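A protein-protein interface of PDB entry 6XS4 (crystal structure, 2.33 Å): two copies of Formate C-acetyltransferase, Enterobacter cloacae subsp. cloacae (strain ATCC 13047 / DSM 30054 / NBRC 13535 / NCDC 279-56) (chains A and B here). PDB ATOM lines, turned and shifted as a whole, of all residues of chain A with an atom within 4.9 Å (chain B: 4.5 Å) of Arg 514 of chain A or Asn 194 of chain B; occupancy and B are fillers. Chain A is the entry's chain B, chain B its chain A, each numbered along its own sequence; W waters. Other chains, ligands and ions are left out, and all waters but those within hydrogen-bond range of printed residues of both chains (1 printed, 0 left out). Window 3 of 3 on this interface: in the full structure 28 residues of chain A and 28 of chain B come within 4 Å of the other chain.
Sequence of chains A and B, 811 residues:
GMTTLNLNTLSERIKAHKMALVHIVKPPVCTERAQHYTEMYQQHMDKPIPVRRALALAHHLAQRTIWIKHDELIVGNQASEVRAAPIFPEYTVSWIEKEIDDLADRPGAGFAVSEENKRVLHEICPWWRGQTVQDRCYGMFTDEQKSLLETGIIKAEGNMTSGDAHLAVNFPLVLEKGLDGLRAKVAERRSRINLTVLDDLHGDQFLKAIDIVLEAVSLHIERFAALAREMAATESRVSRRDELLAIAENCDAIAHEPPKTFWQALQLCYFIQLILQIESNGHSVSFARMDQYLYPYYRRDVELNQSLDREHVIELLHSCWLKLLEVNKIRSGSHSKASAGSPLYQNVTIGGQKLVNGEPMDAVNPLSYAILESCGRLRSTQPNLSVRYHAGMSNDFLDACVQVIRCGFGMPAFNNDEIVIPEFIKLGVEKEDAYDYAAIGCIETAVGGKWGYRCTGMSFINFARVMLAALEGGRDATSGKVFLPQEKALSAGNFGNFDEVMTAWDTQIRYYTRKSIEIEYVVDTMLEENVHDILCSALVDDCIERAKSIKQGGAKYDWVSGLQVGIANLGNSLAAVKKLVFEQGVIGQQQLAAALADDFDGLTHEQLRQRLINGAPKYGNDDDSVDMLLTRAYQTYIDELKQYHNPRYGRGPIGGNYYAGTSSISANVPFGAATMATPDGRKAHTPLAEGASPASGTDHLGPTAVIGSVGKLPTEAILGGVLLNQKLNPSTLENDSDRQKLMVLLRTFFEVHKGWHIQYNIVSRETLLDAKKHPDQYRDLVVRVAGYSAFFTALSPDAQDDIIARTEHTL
OD1 of Asn 194 of chain B sits at hydrogen-bond distance from NH1 of Arg 514 of chain A (3.3 Å).
OD1 of Asn 194 of chain B sits at hydrogen-bond distance from OG1 of Thr 196 of chain B (2.5 Å). OD2 of Asp 200 of chain B lies within hydrogen-bond range of N of Asn 194 of chain B, 3.1 Å away. NH2 of Arg 514 of chain A is in salt-bridge range of OE2 of Glu 518 of chain A (3.1 Å). NZ of Lys 515 of chain A lies within salt-bridge range of OE1 of Glu 518 of chain A, 3.3 Å away.
Ile 517 of chain A touches Thr 196 of chain B. Glu 518 of chain A touches Leu 195 of chain B (CG to CB, 3.8 Å). Glu 518 of chain A touches Thr 196 of chain B. Thr 196 of chain B touches Tyr 644 of chain A.
Of chain B, only Asn 194 comes within 4 Å of Arg 514 of chain A. Of the printed residues of chain B, Ile 517 of chain A touches Thr 196. Printed residues of chain B within 4 Å of Glu 518 of chain A: Leu 195 and Thr 196. Printed residues of chain B within 4 Å of Tyr 644 of chain A: Thr 196. Asn 194 of chain B touches just one residue of chain A: Arg 514. Of the printed residues of chain A, Thr 196 of chain B touches Ile 517 (3.7 Å), Glu 518 (3.6 Å) and Tyr 644 (3.5 Å). Asp 200 of chain B touches none of the printed residues of chain A. The nearest residue of chain B that does not touch Arg 514 of chain A is Thr 196 of chain B (4.2 Å).
Of the 10 printed residues of chain A, 4 touch a printed residue of chain B. Hydrophobic or aromatic side chains of chain A within 4 Å of the printed part of chain B: Ile 517 and Tyr 644. Of the 7 printed residues of chain B, 3 touch a printed residue of chain A. Printed residues of chain B that touch a printed residue of chain A: Asn 194, Leu 195 and Thr 196. Among the printed residues, 5 pairs touch across the chains. Among the printed residues, no Asp or Glu carboxylate lies within 4 Å of a Lys or Arg side-chain nitrogen of the other chain.
No position is printed for both chains.
Water W1 lies within hydrogen-bond range of O of Leu 195 of chain B (2.7 Å) and O of Glu 518 of chain A (2.8 Å).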
ATOM      1  N   ARG A 510      29.104   6.332  -8.013  1.00  0.00           N
ATOM      2  CA  ARG A 510      28.559   7.679  -8.148  1.00  0.00           C
ATOM      3  C   ARG A 510      28.336   8.032  -9.613  1.00  0.00           C
ATOM      4  O   ARG A 510      27.365   8.720  -9.949  1.00  0.00           O
ATOM      5  CB  ARG A 510      29.484   8.692  -7.477  1.00  0.00           C
ATOM      6  CG  ARG A 510      29.257   8.793  -5.978  1.00  0.00           C
ATOM      7  CD  ARG A 510      30.194   9.784  -5.308  1.00  0.00           C
ATOM      8  NE  ARG A 510      30.265   9.536  -3.870  1.00  0.00           N
ATOM      9  CZ  ARG A 510      29.474  10.100  -2.960  1.00  0.00           C
ATOM     10  NH1 ARG A 510      28.539  10.971  -3.318  1.00  0.00           N
ATOM     11  NH2 ARG A 510      29.625   9.792  -1.681  1.00  0.00           N
ATOM     12  N   TYR A 511      29.215   7.561 -10.499  1.00  0.00           N
ATOM     13  CA  TYR A 511      29.022   7.788 -11.927  1.00  0.00           C
ATOM     14  C   TYR A 511      27.781   7.059 -12.433  1.00  0.00           C
ATOM     15  O   TYR A 511      26.894   7.670 -13.044  1.00  0.00           O
ATOM     16  CB  TYR A 511      30.262   7.338 -12.699  1.00  0.00           C
ATOM     17  CG  TYR A 511      30.013   7.110 -14.172  1.00  0.00           C
ATOM     18  CD1 TYR A 511      29.679   5.850 -14.653  1.00  0.00           C
ATOM     19  CD2 TYR A 511      30.106   8.156 -15.081  1.00  0.00           C
ATOM     20  CE1 TYR A 511      29.443   5.640 -15.998  1.00  0.00           C
ATOM     21  CE2 TYR A 511      29.874   7.955 -16.426  1.00  0.00           C
ATOM     22  CZ  TYR A 511      29.543   6.696 -16.879  1.00  0.00           C
ATOM     23  OH  TYR A 511      29.308   6.487 -18.216  1.00  0.00           O
ATOM     24  N   TYR A 512      27.701   5.749 -12.190  1.00  0.00           N
ATOM     25  CA  TYR A 512      26.554   4.983 -12.668  1.00  0.00           C
ATOM     26  C   TYR A 512      25.259   5.468 -12.033  1.00  0.00           C
ATOM     27  O   TYR A 512      24.194   5.386 -12.657  1.00  0.00           O
ATOM     28  CB  TYR A 512      26.767   3.493 -12.394  1.00  0.00           C
ATOM     29  CG  TYR A 512      27.804   2.872 -13.302  1.00  0.00           C
ATOM     30  CD1 TYR A 512      27.483   2.515 -14.606  1.00  0.00           C
ATOM     31  CD2 TYR A 512      29.104   2.656 -12.864  1.00  0.00           C
ATOM     32  CE1 TYR A 512      28.425   1.956 -15.446  1.00  0.00           C
ATOM     33  CE2 TYR A 512      30.054   2.096 -13.698  1.00  0.00           C
ATOM     34  CZ  TYR A 512      29.709   1.748 -14.987  1.00  0.00           C
ATOM     35  OH  TYR A 512      30.649   1.191 -15.822  1.00  0.00           O
ATOM     36  N   THR A 513      25.328   5.985 -10.805  1.00  0.00           N
ATOM     37  CA  THR A 513      24.135   6.534 -10.168  1.00  0.00           C
ATOM     38  C   THR A 513      23.619   7.745 -10.938  1.00  0.00           C
ATOM     39  O   THR A 513      22.416   7.868 -11.188  1.00  0.00           O
ATOM     40  CB  THR A 513      24.438   6.900  -8.713  1.00  0.00           C
ATOM     41  OG1 THR A 513      24.761   5.712  -7.978  1.00  0.00           O
ATOM     42  CG2 THR A 513      23.240   7.575  -8.062  1.00  0.00           C
ATOM     43  N   ARG A 514      24.521   8.653 -11.325  1.00  0.00           N
ATOM     44  CA  ARG A 514      24.099   9.812 -12.106  1.00  0.00           C
ATOM     45  C   ARG A 514      23.501   9.383 -13.440  1.00  0.00           C
ATOM     46  O   ARG A 514      22.467   9.912 -13.865  1.00  0.00           O
ATOM     47  CB  ARG A 514      25.275  10.765 -12.331  1.00  0.00           C
ATOM     48  CG  ARG A 514      24.901  12.006 -13.131  1.00  0.00           C
ATOM     49  CD  ARG A 514      26.035  13.017 -13.193  1.00  0.00           C
ATOM     50  NE  ARG A 514      25.684  14.275 -12.535  1.00  0.00           N
ATOM     51  CZ  ARG A 514      24.972  15.249 -13.098  1.00  0.00           C
ATOM     52  NH1 ARG A 514      24.709  16.352 -12.413  1.00  0.00           N
ATOM     53  NH2 ARG A 514      24.517  15.123 -14.339  1.00  0.00           N
ATOM     54  N   LYS A 515      24.134   8.420 -14.115  1.00  0.00           N
ATOM     55  CA  LYS A 515      23.609   7.947 -15.390  1.00  0.00           C
ATOM     56  C   LYS A 515      22.225   7.332 -15.223  1.00  0.00           C
ATOM     57  O   LYS A 515      21.325   7.585 -16.031  1.00  0.00           O
ATOM     58  CB  LYS A 515      24.571   6.933 -16.013  1.00  0.00           C
ATOM     59  CG  LYS A 515      25.952   7.497 -16.343  1.00  0.00           C
ATOM     60  CD  LYS A 515      25.878   8.631 -17.364  1.00  0.00           C
ATOM     61  CE  LYS A 515      27.067   9.566 -17.245  1.00  0.00           C
ATOM     62  NZ  LYS A 515      26.697  10.952 -17.632  1.00  0.00           N
ATOM     63  N   SER A 516      22.035   6.522 -14.180  1.00  0.00           N
ATOM     64  CA  SER A 516      20.727   5.915 -13.960  1.00  0.00           C
ATOM     65  C   SER A 516      19.649   6.983 -13.827  1.00  0.00           C
ATOM     66  O   SER A 516      18.540   6.825 -14.351  1.00  0.00           O
ATOM     67  CB  SER A 516      20.761   5.025 -12.716  1.00  0.00           C
ATOM     68  OG  SER A 516      20.813   5.801 -11.532  1.00  0.00           O
ATOM     69  N   ILE A 517      19.961   8.087 -13.144  1.00  0.00           N
ATOM     70  CA  ILE A 517      18.965   9.133 -12.939  1.00  0.00           C
ATOM     71  C   ILE A 517      18.730   9.913 -14.229  1.00  0.00           C
ATOM     72  O   ILE A 517      17.597  10.301 -14.536  1.00  0.00           O
ATOM     73  CB  ILE A 517      19.391  10.059 -11.786  1.00  0.00           C
ATOM     74  CG1 ILE A 517      19.489   9.273 -10.474  1.00  0.00           C
ATOM     75  CG2 ILE A 517      18.411  11.218 -11.637  1.00  0.00           C
ATOM     76  CD1 ILE A 517      18.209   8.559 -10.071  1.00  0.00           C
ATOM     77  N   GLU A 518      19.790  10.161 -15.003  1.00  0.00           N
ATOM     78  CA  GLU A 518      19.608  10.787 -16.307  1.00  0.00           C
ATOM     79  C   GLU A 518      18.714   9.932 -17.197  1.00  0.00           C
ATOM     80  O   GLU A 518      17.854  10.453 -17.916  1.00  0.00           O
ATOM     81  CB  GLU A 518      20.962  11.019 -16.981  1.00  0.00           C
ATOM     82  CG  GLU A 518      21.832  12.061 -16.303  1.00  0.00           C
ATOM     83  CD  GLU A 518      23.189  12.195 -16.963  1.00  0.00           C
ATOM     84  OE1 GLU A 518      23.430  11.497 -17.970  1.00  0.00           O
ATOM     85  OE2 GLU A 518      24.011  12.997 -16.473  1.00  0.00           O
ATOM     86  N   TYR A 644      19.880  14.520  -5.851  1.00  0.00           N
ATOM     87  CA  TYR A 644      18.933  14.575  -6.949  1.00  0.00           C
ATOM     88  C   TYR A 644      17.510  14.680  -6.421  1.00  0.00           C
ATOM     89  O   TYR A 644      17.224  14.372  -5.261  1.00  0.00           O
ATOM     90  CB  TYR A 644      19.049  13.334  -7.847  1.00  0.00           C
ATOM     91  CG  TYR A 644      20.451  13.051  -8.330  1.00  0.00           C
ATOM     92  CD1 TYR A 644      21.263  12.130  -7.674  1.00  0.00           C
ATOM     93  CD2 TYR A 644      20.964  13.699  -9.442  1.00  0.00           C
ATOM     94  CE1 TYR A 644      22.546  11.868  -8.114  1.00  0.00           C
ATOM     95  CE2 TYR A 644      22.246  13.444  -9.889  1.00  0.00           C
ATOM     96  CZ  TYR A 644      23.032  12.527  -9.222  1.00  0.00           C
ATOM     97  OH  TYR A 644      24.309  12.272  -9.668  1.00  0.00           O
ATOM     98  N   ARG B 192      26.375  23.937 -19.362  1.00  0.00           N
ATOM     99  CA  ARG B 192      25.747  24.167 -18.070  1.00  0.00           C
ATOM    100  C   ARG B 192      24.436  23.408 -17.914  1.00  0.00           C
ATOM    101  O   ARG B 192      23.674  23.689 -16.983  1.00  0.00           O
ATOM    102  CB  ARG B 192      25.514  25.667 -17.860  1.00  0.00           C
ATOM    103  CG  ARG B 192      26.797  26.459 -17.679  1.00  0.00           C
ATOM    104  CD  ARG B 192      26.532  27.940 -17.431  1.00  0.00           C
ATOM    105  NE  ARG B 192      26.332  28.691 -18.673  1.00  0.00           N
ATOM    106  CZ  ARG B 192      25.230  29.372 -18.991  1.00  0.00           C
ATOM    107  NH1 ARG B 192      24.194  29.426 -18.165  1.00  0.00           N
ATOM    108  NH2 ARG B 192      25.173  30.017 -20.150  1.00  0.00           N
ATOM    109  N   ILE B 193      24.158  22.455 -18.800  1.00  0.00           N
ATOM    110  CA  ILE B 193      22.945  21.651 -18.714  1.00  0.00           C
ATOM    111  C   ILE B 193      23.158  20.531 -17.705  1.00  0.00           C
ATOM    112  O   ILE B 193      24.183  19.839 -17.737  1.00  0.00           O
ATOM    113  CB  ILE B 193      22.571  21.081 -20.093  1.00  0.00           C
ATOM    114  CG1 ILE B 193      21.955  22.167 -20.982  1.00  0.00           C
ATOM    115  CG2 ILE B 193      21.633  19.882 -19.946  1.00  0.00           C
ATOM    116  CD1 ILE B 193      20.596  22.664 -20.521  1.00  0.00           C
ATOM    117  N   ASN B 194      22.186  20.344 -16.814  1.00  0.00           N
ATOM    118  CA  ASN B 194      22.155  19.223 -15.879  1.00  0.00           C
ATOM    119  C   ASN B 194      20.996  18.322 -16.292  1.00  0.00           C
ATOM    120  O   ASN B 194      19.828  18.698 -16.142  1.00  0.00           O
ATOM    121  CB  ASN B 194      21.996  19.712 -14.441  1.00  0.00           C
ATOM    122  CG  ASN B 194      22.144  18.596 -13.421  1.00  0.00           C
ATOM    123  OD1 ASN B 194      21.907  17.427 -13.720  1.00  0.00           O
ATOM    124  ND2 ASN B 194      22.536  18.958 -12.206  1.00  0.00           N
ATOM    125  N   LEU B 195      21.315  17.143 -16.821  1.00  0.00           N
ATOM    126  CA  LEU B 195      20.300  16.248 -17.365  1.00  0.00           C
ATOM    127  C   LEU B 195      19.498  15.529 -16.285  1.00  0.00           C
ATOM    128  O   LEU B 195      18.678  14.665 -16.620  1.00  0.00           O
ATOM    129  CB  LEU B 195      20.951  15.228 -18.300  1.00  0.00           C
ATOM    130  CG  LEU B 195      21.484  15.801 -19.616  1.00  0.00           C
ATOM    131  CD1 LEU B 195      22.312  14.760 -20.353  1.00  0.00           C
ATOM    132  CD2 LEU B 195      20.344  16.304 -20.499  1.00  0.00           C
ATOM    133  N   THR B 196      19.720  15.855 -15.010  1.00  0.00           N
ATOM    134  CA  THR B 196      18.872  15.392 -13.919  1.00  0.00           C
ATOM    135  C   THR B 196      17.971  16.508 -13.396  1.00  0.00           C
ATOM    136  O   THR B 196      17.401  16.385 -12.307  1.00  0.00           O
ATOM    137  CB  THR B 196      19.725  14.819 -12.786  1.00  0.00           C
ATOM    138  OG1 THR B 196      20.573  15.839 -12.245  1.00  0.00           O
ATOM    139  CG2 THR B 196      20.579  13.670 -13.302  1.00  0.00           C
ATOM    140  N   VAL B 197      17.836  17.591 -14.158  1.00  0.00           N
ATOM    141  CA  VAL B 197      16.954  18.707 -13.838  1.00  0.00           C
ATOM    142  C   VAL B 197      15.963  18.837 -14.986  1.00  0.00           C
ATOM    143  O   VAL B 197      16.369  18.971 -16.147  1.00  0.00           O
ATOM    144  CB  VAL B 197      17.734  20.015 -13.635  1.00  0.00           C
ATOM    145  CG1 VAL B 197      16.776  21.181 -13.416  1.00  0.00           C
ATOM    146  CG2 VAL B 197      18.708  19.874 -12.469  1.00  0.00           C
ATOM    147  N   ASP B 200      16.150  21.540 -17.615  1.00  0.00           N
ATOM    148  CA  ASP B 200      17.373  21.422 -18.401  1.00  0.00           C
ATOM    149  C   ASP B 200      17.289  20.293 -19.420  1.00  0.00           C
ATOM    150  O   ASP B 200      17.957  20.351 -20.457  1.00  0.00           O
ATOM    151  CB  ASP B 200      18.574  21.204 -17.477  1.00  0.00           C
ATOM    152  CG  ASP B 200      19.014  22.477 -16.778  1.00  0.00           C
ATOM    153  OD1 ASP B 200      18.327  23.508 -16.928  1.00  0.00           O
ATOM    154  OD2 ASP B 200      20.053  22.445 -16.082  1.00  0.00           O
HETATM  155  O   HOH W   1      18.203  13.073 -18.694  1.00  0.00           O
